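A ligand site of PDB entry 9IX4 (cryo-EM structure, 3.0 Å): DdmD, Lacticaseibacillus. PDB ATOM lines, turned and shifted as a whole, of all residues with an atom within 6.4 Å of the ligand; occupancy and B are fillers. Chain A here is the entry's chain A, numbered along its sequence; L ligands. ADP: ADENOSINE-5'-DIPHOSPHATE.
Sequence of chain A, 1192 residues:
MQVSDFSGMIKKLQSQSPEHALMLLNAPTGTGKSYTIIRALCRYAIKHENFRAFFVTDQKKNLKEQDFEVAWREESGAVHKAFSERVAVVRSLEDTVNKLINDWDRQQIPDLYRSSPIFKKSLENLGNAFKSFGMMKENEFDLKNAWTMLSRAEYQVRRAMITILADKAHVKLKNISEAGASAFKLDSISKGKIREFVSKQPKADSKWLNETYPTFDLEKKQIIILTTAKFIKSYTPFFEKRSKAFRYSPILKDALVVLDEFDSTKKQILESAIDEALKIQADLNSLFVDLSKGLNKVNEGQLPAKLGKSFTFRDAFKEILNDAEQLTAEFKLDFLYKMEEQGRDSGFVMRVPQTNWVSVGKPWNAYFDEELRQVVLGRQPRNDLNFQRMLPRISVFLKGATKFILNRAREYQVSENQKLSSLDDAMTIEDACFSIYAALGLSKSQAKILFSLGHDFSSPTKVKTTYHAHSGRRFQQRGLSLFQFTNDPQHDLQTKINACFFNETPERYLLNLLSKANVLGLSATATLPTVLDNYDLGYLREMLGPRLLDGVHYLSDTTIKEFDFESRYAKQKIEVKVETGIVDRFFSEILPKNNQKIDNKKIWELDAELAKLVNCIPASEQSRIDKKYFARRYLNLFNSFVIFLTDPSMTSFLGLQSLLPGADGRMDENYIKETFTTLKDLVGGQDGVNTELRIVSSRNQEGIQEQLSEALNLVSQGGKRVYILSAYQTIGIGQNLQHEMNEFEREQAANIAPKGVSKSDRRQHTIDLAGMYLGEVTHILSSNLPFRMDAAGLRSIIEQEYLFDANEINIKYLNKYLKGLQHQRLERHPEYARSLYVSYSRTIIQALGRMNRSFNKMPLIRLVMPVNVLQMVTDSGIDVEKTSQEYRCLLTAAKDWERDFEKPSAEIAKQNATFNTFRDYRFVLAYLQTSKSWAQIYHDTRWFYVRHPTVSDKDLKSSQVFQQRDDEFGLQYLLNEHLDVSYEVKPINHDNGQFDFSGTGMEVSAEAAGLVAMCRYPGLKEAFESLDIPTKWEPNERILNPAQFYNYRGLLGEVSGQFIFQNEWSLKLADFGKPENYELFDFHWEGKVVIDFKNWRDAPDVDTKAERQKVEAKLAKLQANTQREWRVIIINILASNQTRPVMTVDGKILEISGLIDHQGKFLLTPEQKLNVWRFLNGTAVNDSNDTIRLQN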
ATOM      1  N   MET A   1      -6.588  10.297  -5.918  1.00  0.00           N
ATOM      2  CA  MET A   1      -5.555  10.244  -4.892  1.00  0.00           C
ATOM      3  C   MET A   1      -4.801   8.921  -4.984  1.00  0.00           C
ATOM      4  O   MET A   1      -5.416   7.858  -5.046  1.00  0.00           O
ATOM      5  CB  MET A   1      -6.162  10.419  -3.500  1.00  0.00           C
ATOM      6  CG  MET A   1      -6.879  11.743  -3.320  1.00  0.00           C
ATOM      7  SD  MET A   1      -7.630  11.911  -1.695  1.00  0.00           S
ATOM      8  CE  MET A   1      -6.182  12.220  -0.700  1.00  0.00           C
ATOM      9  N   ALA A  27      -8.391  16.863   3.060  1.00  0.00           N
ATOM     10  CA  ALA A  27      -8.648  16.679   1.649  1.00  0.00           C
ATOM     11  C   ALA A  27     -10.141  16.905   1.461  1.00  0.00           C
ATOM     12  O   ALA A  27     -10.954  16.349   2.224  1.00  0.00           O
ATOM     13  CB  ALA A  27      -8.246  15.286   1.157  1.00  0.00           C
ATOM     14  N   PRO A  28     -10.539  17.707   0.478  1.00  0.00           N
ATOM     15  CA  PRO A  28     -11.964  17.988   0.289  1.00  0.00           C
ATOM     16  C   PRO A  28     -12.744  16.712   0.018  1.00  0.00           C
ATOM     17  O   PRO A  28     -12.229  15.737  -0.521  1.00  0.00           O
ATOM     18  CB  PRO A  28     -11.992  18.923  -0.927  1.00  0.00           C
ATOM     19  CG  PRO A  28     -10.669  18.723  -1.593  1.00  0.00           C
ATOM     20  CD  PRO A  28      -9.701  18.390  -0.521  1.00  0.00           C
ATOM     21  N   THR A  29     -14.016  16.732   0.424  1.00  0.00           N
ATOM     22  CA  THR A  29     -14.868  15.564   0.286  1.00  0.00           C
ATOM     23  C   THR A  29     -15.106  15.247  -1.187  1.00  0.00           C
ATOM     24  O   THR A  29     -14.916  16.085  -2.072  1.00  0.00           O
ATOM     25  CB  THR A  29     -16.218  15.787   0.977  1.00  0.00           C
ATOM     26  OG1 THR A  29     -17.006  14.593   0.877  1.00  0.00           O
ATOM     27  CG2 THR A  29     -16.952  16.925   0.323  1.00  0.00           C
ATOM     28  N   GLY A  30     -15.518  14.012  -1.444  1.00  0.00           N
ATOM     29  CA  GLY A  30     -15.714  13.531  -2.782  1.00  0.00           C
ATOM     30  C   GLY A  30     -14.476  12.989  -3.445  1.00  0.00           C
ATOM     31  O   GLY A  30     -14.582  12.261  -4.439  1.00  0.00           O
ATOM     32  N   THR A  31     -13.299  13.294  -2.915  1.00  0.00           N
ATOM     33  CA  THR A  31     -12.068  12.687  -3.374  1.00  0.00           C
ATOM     34  C   THR A  31     -11.843  11.380  -2.631  1.00  0.00           C
ATOM     35  O   THR A  31     -12.503  11.085  -1.627  1.00  0.00           O
ATOM     36  CB  THR A  31     -10.882  13.637  -3.181  1.00  0.00           C
ATOM     37  OG1 THR A  31     -10.510  13.652  -1.799  1.00  0.00           O
ATOM     38  CG2 THR A  31     -11.260  15.040  -3.602  1.00  0.00           C
ATOM     39  N   GLY A  32     -10.899  10.587  -3.129  1.00  0.00           N
ATOM     40  CA  GLY A  32     -10.722   9.255  -2.584  1.00  0.00           C
ATOM     41  C   GLY A  32      -9.990   9.201  -1.263  1.00  0.00           C
ATOM     42  O   GLY A  32      -8.890   8.668  -1.192  1.00  0.00           O
ATOM     43  N   LYS A  33     -10.590   9.745  -0.197  1.00  0.00           N
ATOM     44  CA  LYS A  33     -10.000   9.551   1.118  1.00  0.00           C
ATOM     45  C   LYS A  33     -10.292   8.151   1.642  1.00  0.00           C
ATOM     46  O   LYS A  33      -9.375   7.368   1.898  1.00  0.00           O
ATOM     47  CB  LYS A  33     -10.509  10.607   2.111  1.00  0.00           C
ATOM     48  CG  LYS A  33     -10.079  12.031   1.824  1.00  0.00           C
ATOM     49  CD  LYS A  33     -10.434  12.928   2.998  1.00  0.00           C
ATOM     50  CE  LYS A  33     -11.933  13.011   3.204  1.00  0.00           C
ATOM     51  NZ  LYS A  33     -12.635  13.635   2.051  1.00  0.00           N
ATOM     52  N   SER A  34     -11.575   7.826   1.781  1.00  0.00           N
ATOM     53  CA  SER A  34     -11.959   6.523   2.315  1.00  0.00           C
ATOM     54  C   SER A  34     -11.509   5.380   1.418  1.00  0.00           C
ATOM     55  O   SER A  34     -10.972   4.381   1.903  1.00  0.00           O
ATOM     56  CB  SER A  34     -13.463   6.461   2.532  1.00  0.00           C
ATOM     57  OG  SER A  34     -13.929   7.623   3.205  1.00  0.00           O
ATOM     58  N   TYR A  35     -11.700   5.529   0.121  1.00  0.00           N
ATOM     59  CA  TYR A  35     -11.313   4.481  -0.799  1.00  0.00           C
ATOM     60  C   TYR A  35      -9.850   4.169  -0.691  1.00  0.00           C
ATOM     61  O   TYR A  35      -9.468   3.043  -0.423  1.00  0.00           O
ATOM     62  CB  TYR A  35     -11.601   4.925  -2.220  1.00  0.00           C
ATOM     63  CG  TYR A  35     -11.378   3.859  -3.244  1.00  0.00           C
ATOM     64  CD1 TYR A  35     -11.938   2.598  -3.093  1.00  0.00           C
ATOM     65  CD2 TYR A  35     -10.608   4.106  -4.364  1.00  0.00           C
ATOM     66  CE1 TYR A  35     -11.731   1.612  -4.030  1.00  0.00           C
ATOM     67  CE2 TYR A  35     -10.403   3.125  -5.313  1.00  0.00           C
ATOM     68  CZ  TYR A  35     -10.964   1.883  -5.141  1.00  0.00           C
ATOM     69  OH  TYR A  35     -10.766   0.908  -6.087  1.00  0.00           O
ATOM     70  N   THR A  36      -9.017   5.175  -0.883  1.00  0.00           N
ATOM     71  CA  THR A  36      -7.582   4.949  -0.871  1.00  0.00           C
ATOM     72  C   THR A  36      -7.055   4.578   0.495  1.00  0.00           C
ATOM     73  O   THR A  36      -6.083   3.821   0.576  1.00  0.00           O
ATOM     74  CB  THR A  36      -6.847   6.179  -1.406  1.00  0.00           C
ATOM     75  OG1 THR A  36      -7.169   7.310  -0.598  1.00  0.00           O
ATOM     76  CG2 THR A  36      -7.248   6.450  -2.831  1.00  0.00           C
ATOM     77  N   ARG A  39      -7.684   0.906   0.650  1.00  0.00           N
ATOM     78  CA  ARG A  39      -6.725   0.177  -0.172  1.00  0.00           C
ATOM     79  C   ARG A  39      -5.362   0.118   0.502  1.00  0.00           C
ATOM     80  O   ARG A  39      -4.723  -0.939   0.525  1.00  0.00           O
ATOM     81  CB  ARG A  39      -6.608   0.835  -1.547  1.00  0.00           C
ATOM     82  CG  ARG A  39      -7.918   0.953  -2.303  1.00  0.00           C
ATOM     83  CD  ARG A  39      -8.494  -0.399  -2.609  1.00  0.00           C
ATOM     84  NE  ARG A  39      -7.617  -1.174  -3.485  1.00  0.00           N
ATOM     85  CZ  ARG A  39      -7.586  -1.059  -4.804  1.00  0.00           C
ATOM     86  NH1 ARG A  39      -8.354  -0.186  -5.440  1.00  0.00           N
ATOM     87  NH2 ARG A  39      -6.769  -1.833  -5.510  1.00  0.00           N
ATOM     88  N   LYS A  64     -18.069   0.553   5.453  1.00  0.00           N
ATOM     89  CA  LYS A  64     -17.610   0.119   4.136  1.00  0.00           C
ATOM     90  C   LYS A  64     -16.905  -1.237   4.216  1.00  0.00           C
ATOM     91  O   LYS A  64     -15.843  -1.437   3.625  1.00  0.00           O
ATOM     92  CB  LYS A  64     -16.698   1.170   3.503  1.00  0.00           C
ATOM     93  CG  LYS A  64     -17.220   2.582   3.591  1.00  0.00           C
ATOM     94  CD  LYS A  64     -16.207   3.564   3.045  1.00  0.00           C
ATOM     95  CE  LYS A  64     -16.790   4.965   2.978  1.00  0.00           C
ATOM     96  NZ  LYS A  64     -18.195   4.949   2.484  1.00  0.00           N
ATOM     97  N   ASP A  67     -16.395  -2.612   0.890  1.00  0.00           N
ATOM     98  CA  ASP A  67     -15.240  -2.021   0.238  1.00  0.00           C
ATOM     99  C   ASP A  67     -13.944  -2.642   0.742  1.00  0.00           C
ATOM    100  O   ASP A  67     -13.012  -2.869  -0.027  1.00  0.00           O
ATOM    101  CB  ASP A  67     -15.237  -0.503   0.460  1.00  0.00           C
ATOM    102  CG  ASP A  67     -14.529   0.240  -0.643  1.00  0.00           C
ATOM    103  OD1 ASP A  67     -13.970  -0.417  -1.542  1.00  0.00           O
ATOM    104  OD2 ASP A  67     -14.541   1.484  -0.617  1.00  0.00           O
ATOM    105  N   ASP A 260     -12.047   7.989  10.543  1.00  0.00           N
ATOM    106  CA  ASP A 260     -12.462   8.361   9.198  1.00  0.00           C
ATOM    107  C   ASP A 260     -13.122   9.732   9.157  1.00  0.00           C
ATOM    108  O   ASP A 260     -13.128  10.381   8.104  1.00  0.00           O
ATOM    109  CB  ASP A 260     -13.417   7.318   8.625  1.00  0.00           C
ATOM    110  CG  ASP A 260     -13.699   7.534   7.156  1.00  0.00           C
ATOM    111  OD1 ASP A 260     -14.577   8.355   6.834  1.00  0.00           O
ATOM    112  OD2 ASP A 260     -13.041   6.891   6.321  1.00  0.00           O
ATOM    113  N   GLU A 261     -13.696  10.194  10.268  1.00  0.00           N
ATOM    114  CA  GLU A 261     -14.220  11.551  10.376  1.00  0.00           C
ATOM    115  C   GLU A 261     -13.653  12.115  11.673  1.00  0.00           C
ATOM    116  O   GLU A 261     -14.286  12.023  12.721  1.00  0.00           O
ATOM    117  CB  GLU A 261     -15.730  11.587  10.349  1.00  0.00           C
ATOM    118  CG  GLU A 261     -16.328  10.930   9.128  1.00  0.00           C
ATOM    119  CD  GLU A 261     -16.311  11.846   7.924  1.00  0.00           C
ATOM    120  OE1 GLU A 261     -15.873  13.001   8.047  1.00  0.00           O
ATOM    121  OE2 GLU A 261     -16.726  11.392   6.839  1.00  0.00           O
ATOM    122  N   ASN A 736     -25.554  10.995  -0.721  1.00  0.00           N
ATOM    123  CA  ASN A 736     -25.378  11.283  -2.136  1.00  0.00           C
ATOM    124  C   ASN A 736     -26.459  12.245  -2.610  1.00  0.00           C
ATOM    125  O   ASN A 736     -27.585  12.242  -2.112  1.00  0.00           O
ATOM    126  CB  ASN A 736     -25.435   9.992  -2.951  1.00  0.00           C
ATOM    127  CG  ASN A 736     -24.447   8.959  -2.463  1.00  0.00           C
ATOM    128  OD1 ASN A 736     -23.236   9.154  -2.573  1.00  0.00           O
ATOM    129  ND2 ASN A 736     -24.956   7.855  -1.926  1.00  0.00           N
ATOM    130  N   ASP A 761     -16.459   5.591 -15.204  1.00  0.00           N
ATOM    131  CA  ASP A 761     -16.249   5.568 -13.769  1.00  0.00           C
ATOM    132  C   ASP A 761     -17.543   5.889 -13.035  1.00  0.00           C
ATOM    133  O   ASP A 761     -18.504   6.415 -13.600  1.00  0.00           O
ATOM    134  CB  ASP A 761     -15.163   6.563 -13.365  1.00  0.00           C
ATOM    135  CG  ASP A 761     -14.650   6.323 -11.954  1.00  0.00           C
ATOM    136  OD1 ASP A 761     -15.024   5.298 -11.349  1.00  0.00           O
ATOM    137  OD2 ASP A 761     -13.881   7.162 -11.449  1.00  0.00           O
ATOM    138  N   ARG A 762     -17.561   5.545 -11.742  1.00  0.00           N
ATOM    139  CA  ARG A 762     -18.734   5.786 -10.918  1.00  0.00           C
ATOM    140  C   ARG A 762     -19.076   7.274 -10.856  1.00  0.00           C
ATOM    141  O   ARG A 762     -20.250   7.651 -10.914  1.00  0.00           O
ATOM    142  CB  ARG A 762     -18.510   5.235  -9.505  1.00  0.00           C
ATOM    143  CG  ARG A 762     -18.447   3.725  -9.446  1.00  0.00           C
ATOM    144  CD  ARG A 762     -18.308   3.229  -8.016  1.00  0.00           C
ATOM    145  NE  ARG A 762     -18.191   1.782  -7.940  1.00  0.00           N
ATOM    146  CZ  ARG A 762     -17.944   1.102  -6.835  1.00  0.00           C
ATOM    147  NH1 ARG A 762     -17.803   1.717  -5.665  1.00  0.00           N
ATOM    148  NH2 ARG A 762     -17.849  -0.226  -6.882  1.00  0.00           N
ATOM    149  N   ARG A 763     -18.058   8.125 -10.765  1.00  0.00           N
ATOM    150  CA  ARG A 763     -18.253   9.565 -10.732  1.00  0.00           C
ATOM    151  C   ARG A 763     -18.402  10.169 -12.125  1.00  0.00           C
ATOM    152  O   ARG A 763     -18.618  11.381 -12.235  1.00  0.00           O
ATOM    153  CB  ARG A 763     -17.076  10.236 -10.011  1.00  0.00           C
ATOM    154  CG  ARG A 763     -16.830   9.725  -8.602  1.00  0.00           C
ATOM    155  CD  ARG A 763     -15.453  10.129  -8.108  1.00  0.00           C
ATOM    156  NE  ARG A 763     -14.386   9.502  -8.875  1.00  0.00           N
ATOM    157  CZ  ARG A 763     -13.097   9.585  -8.573  1.00  0.00           C
ATOM    158  NH1 ARG A 763     -12.679  10.266  -7.523  1.00  0.00           N
ATOM    159  NH2 ARG A 763     -12.212   8.955  -9.348  1.00  0.00           N
ATOM    160  N   ARG A 853     -19.410  15.527  -5.585  1.00  0.00           N
ATOM    161  CA  ARG A 853     -18.964  14.139  -5.562  1.00  0.00           C
ATOM    162  C   ARG A 853     -18.988  13.490  -6.934  1.00  0.00           C
ATOM    163  O   ARG A 853     -18.745  12.283  -7.049  1.00  0.00           O
ATOM    164  CB  ARG A 853     -19.822  13.315  -4.594  1.00  0.00           C
ATOM    165  CG  ARG A 853     -19.673  13.710  -3.131  1.00  0.00           C
ATOM    166  CD  ARG A 853     -20.486  12.784  -2.239  1.00  0.00           C
ATOM    167  NE  ARG A 853     -20.450  13.213  -0.845  1.00  0.00           N
ATOM    168  CZ  ARG A 853     -21.102  12.608   0.135  1.00  0.00           C
ATOM    169  NH1 ARG A 853     -21.823  11.519  -0.084  1.00  0.00           N
ATOM    170  NH2 ARG A 853     -21.037  13.120   1.367  1.00  0.00           N
HETATM  171  PB  ADP L   1     -14.453  10.435   0.728  1.00  0.00           P
HETATM  172  O1B ADP L   1     -15.639   9.641   1.225  1.00  0.00           O
HETATM  173  O2B ADP L   1     -13.583  10.975   1.827  1.00  0.00           O
HETATM  174  O3B ADP L   1     -14.792  11.440  -0.348  1.00  0.00           O
HETATM  175  PA  ADP L   1     -14.056   8.323  -1.100  1.00  0.00           P
HETATM  176  O1A ADP L   1     -12.872   7.559  -1.616  1.00  0.00           O
HETATM  177  O2A ADP L   1     -15.218   7.578  -0.522  1.00  0.00           O
HETATM  178  O3A ADP L   1     -13.509   9.345   0.017  1.00  0.00           O
HETATM  179  O5' ADP L   1     -14.545   9.288  -2.298  1.00  0.00           O
HETATM  180  C5' ADP L   1     -15.898   9.674  -2.458  1.00  0.00           C
HETATM  181  C4' ADP L   1     -16.490   9.015  -3.695  1.00  0.00           C
HETATM  182  O4' ADP L   1     -15.627   9.191  -4.809  1.00  0.00           O
HETATM  183  C3' ADP L   1     -16.666   7.528  -3.496  1.00  0.00           C
HETATM  184  O3' ADP L   1     -17.906   7.097  -4.055  1.00  0.00           O
HETATM  185  C2' ADP L   1     -15.516   6.898  -4.233  1.00  0.00           C
HETATM  186  O2' ADP L   1     -15.855   5.651  -4.845  1.00  0.00           O
HETATM  187  C1' ADP L   1     -15.167   7.922  -5.278  1.00  0.00           C
HETATM  188  N9  ADP L   1     -13.702   7.907  -5.444  1.00  0.00           N
HETATM  189  C8  ADP L   1     -12.844   8.844  -4.995  1.00  0.00           C
HETATM  190  N7  ADP L   1     -11.570   8.496  -5.325  1.00  0.00           N
HETATM  191  C5  ADP L   1     -11.622   7.318  -5.975  1.00  0.00           C
HETATM  192  C6  ADP L   1     -10.657   6.404  -6.591  1.00  0.00           C
HETATM  193  N6  ADP L   1      -9.326   6.680  -6.571  1.00  0.00           N
HETATM  194  N1  ADP L   1     -11.125   5.279  -7.173  1.00  0.00           N
HETATM  195  C2  ADP L   1     -12.442   4.990  -7.198  1.00  0.00           C
HETATM  196  N3  ADP L   1     -13.379   5.786  -6.655  1.00  0.00           N
HETATM  197  C4  ADP L   1     -13.031   6.939  -6.046  1.00  0.00           C
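OG1 of Thr 31 sits at hydrogen-bond distance from SD of Met 1 (3.4 Å). O of Pro 28 lies within hydrogen-bond range of OG1 of Thr 31. The backbone carbonyl oxygen of Lys 33 is in hydrogen-bond range of the side-chain hydroxyl of Thr 36. The backbone carbonyl oxygen of Pro 28 sits at hydrogen-bond distance from the side-chain amino group of Lys 33 (3.3 Å). The backbone carbonyl oxygen of Ala 27 is in hydrogen-bond range of the side-chain amino group of Lys 33 (3.2 Å). The guanidinium group (NH2) of Arg 763 is in salt-bridge range of the side-chain carboxylate (OD2) of Asp 761 (3.2 Å). The side-chain hydroxyl (OH) of Tyr 35 lies within hydrogen-bond range of the guanidinium group (NH1) of Arg 39. The side-chain hydroxyl (OG) of Ser 34 lies within hydrogen-bond range of the side-chain carboxylate (OD2) of Asp 260 (3.3 Å).
Thr 29 touches the ligand. Of the 21 residues printed, 8 come within 4 Å of the ligand.
O3A of the ligand lies close to O of Thr 31 (2.6 Å). The backbone NH (N) of Lys 33 sits at hydrogen-bond distance from an oxygen (O3A) of the ligand, 3.0 Å away. NZ of Lys 33 lies within salt-bridge range of O2B of the ligand (2.8 Å). O3B of the ligand sits at hydrogen-bond distance from N of Gly 30, at 2.9 Å. N of Gly 32 sits close to N7 of the ligand. NH1 of Arg 763 lies close to N7 of the ligand, at 3.0 Å. N of Tyr 35 is in hydrogen-bond range of O1A of the ligand (2.9 Å). O3A of the ligand lies within hydrogen-bond range of N of Ser 34, 3.0 Å away. OG of Ser 34 lies within hydrogen-bond range of O1B of the ligand, 3.3 Å away.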
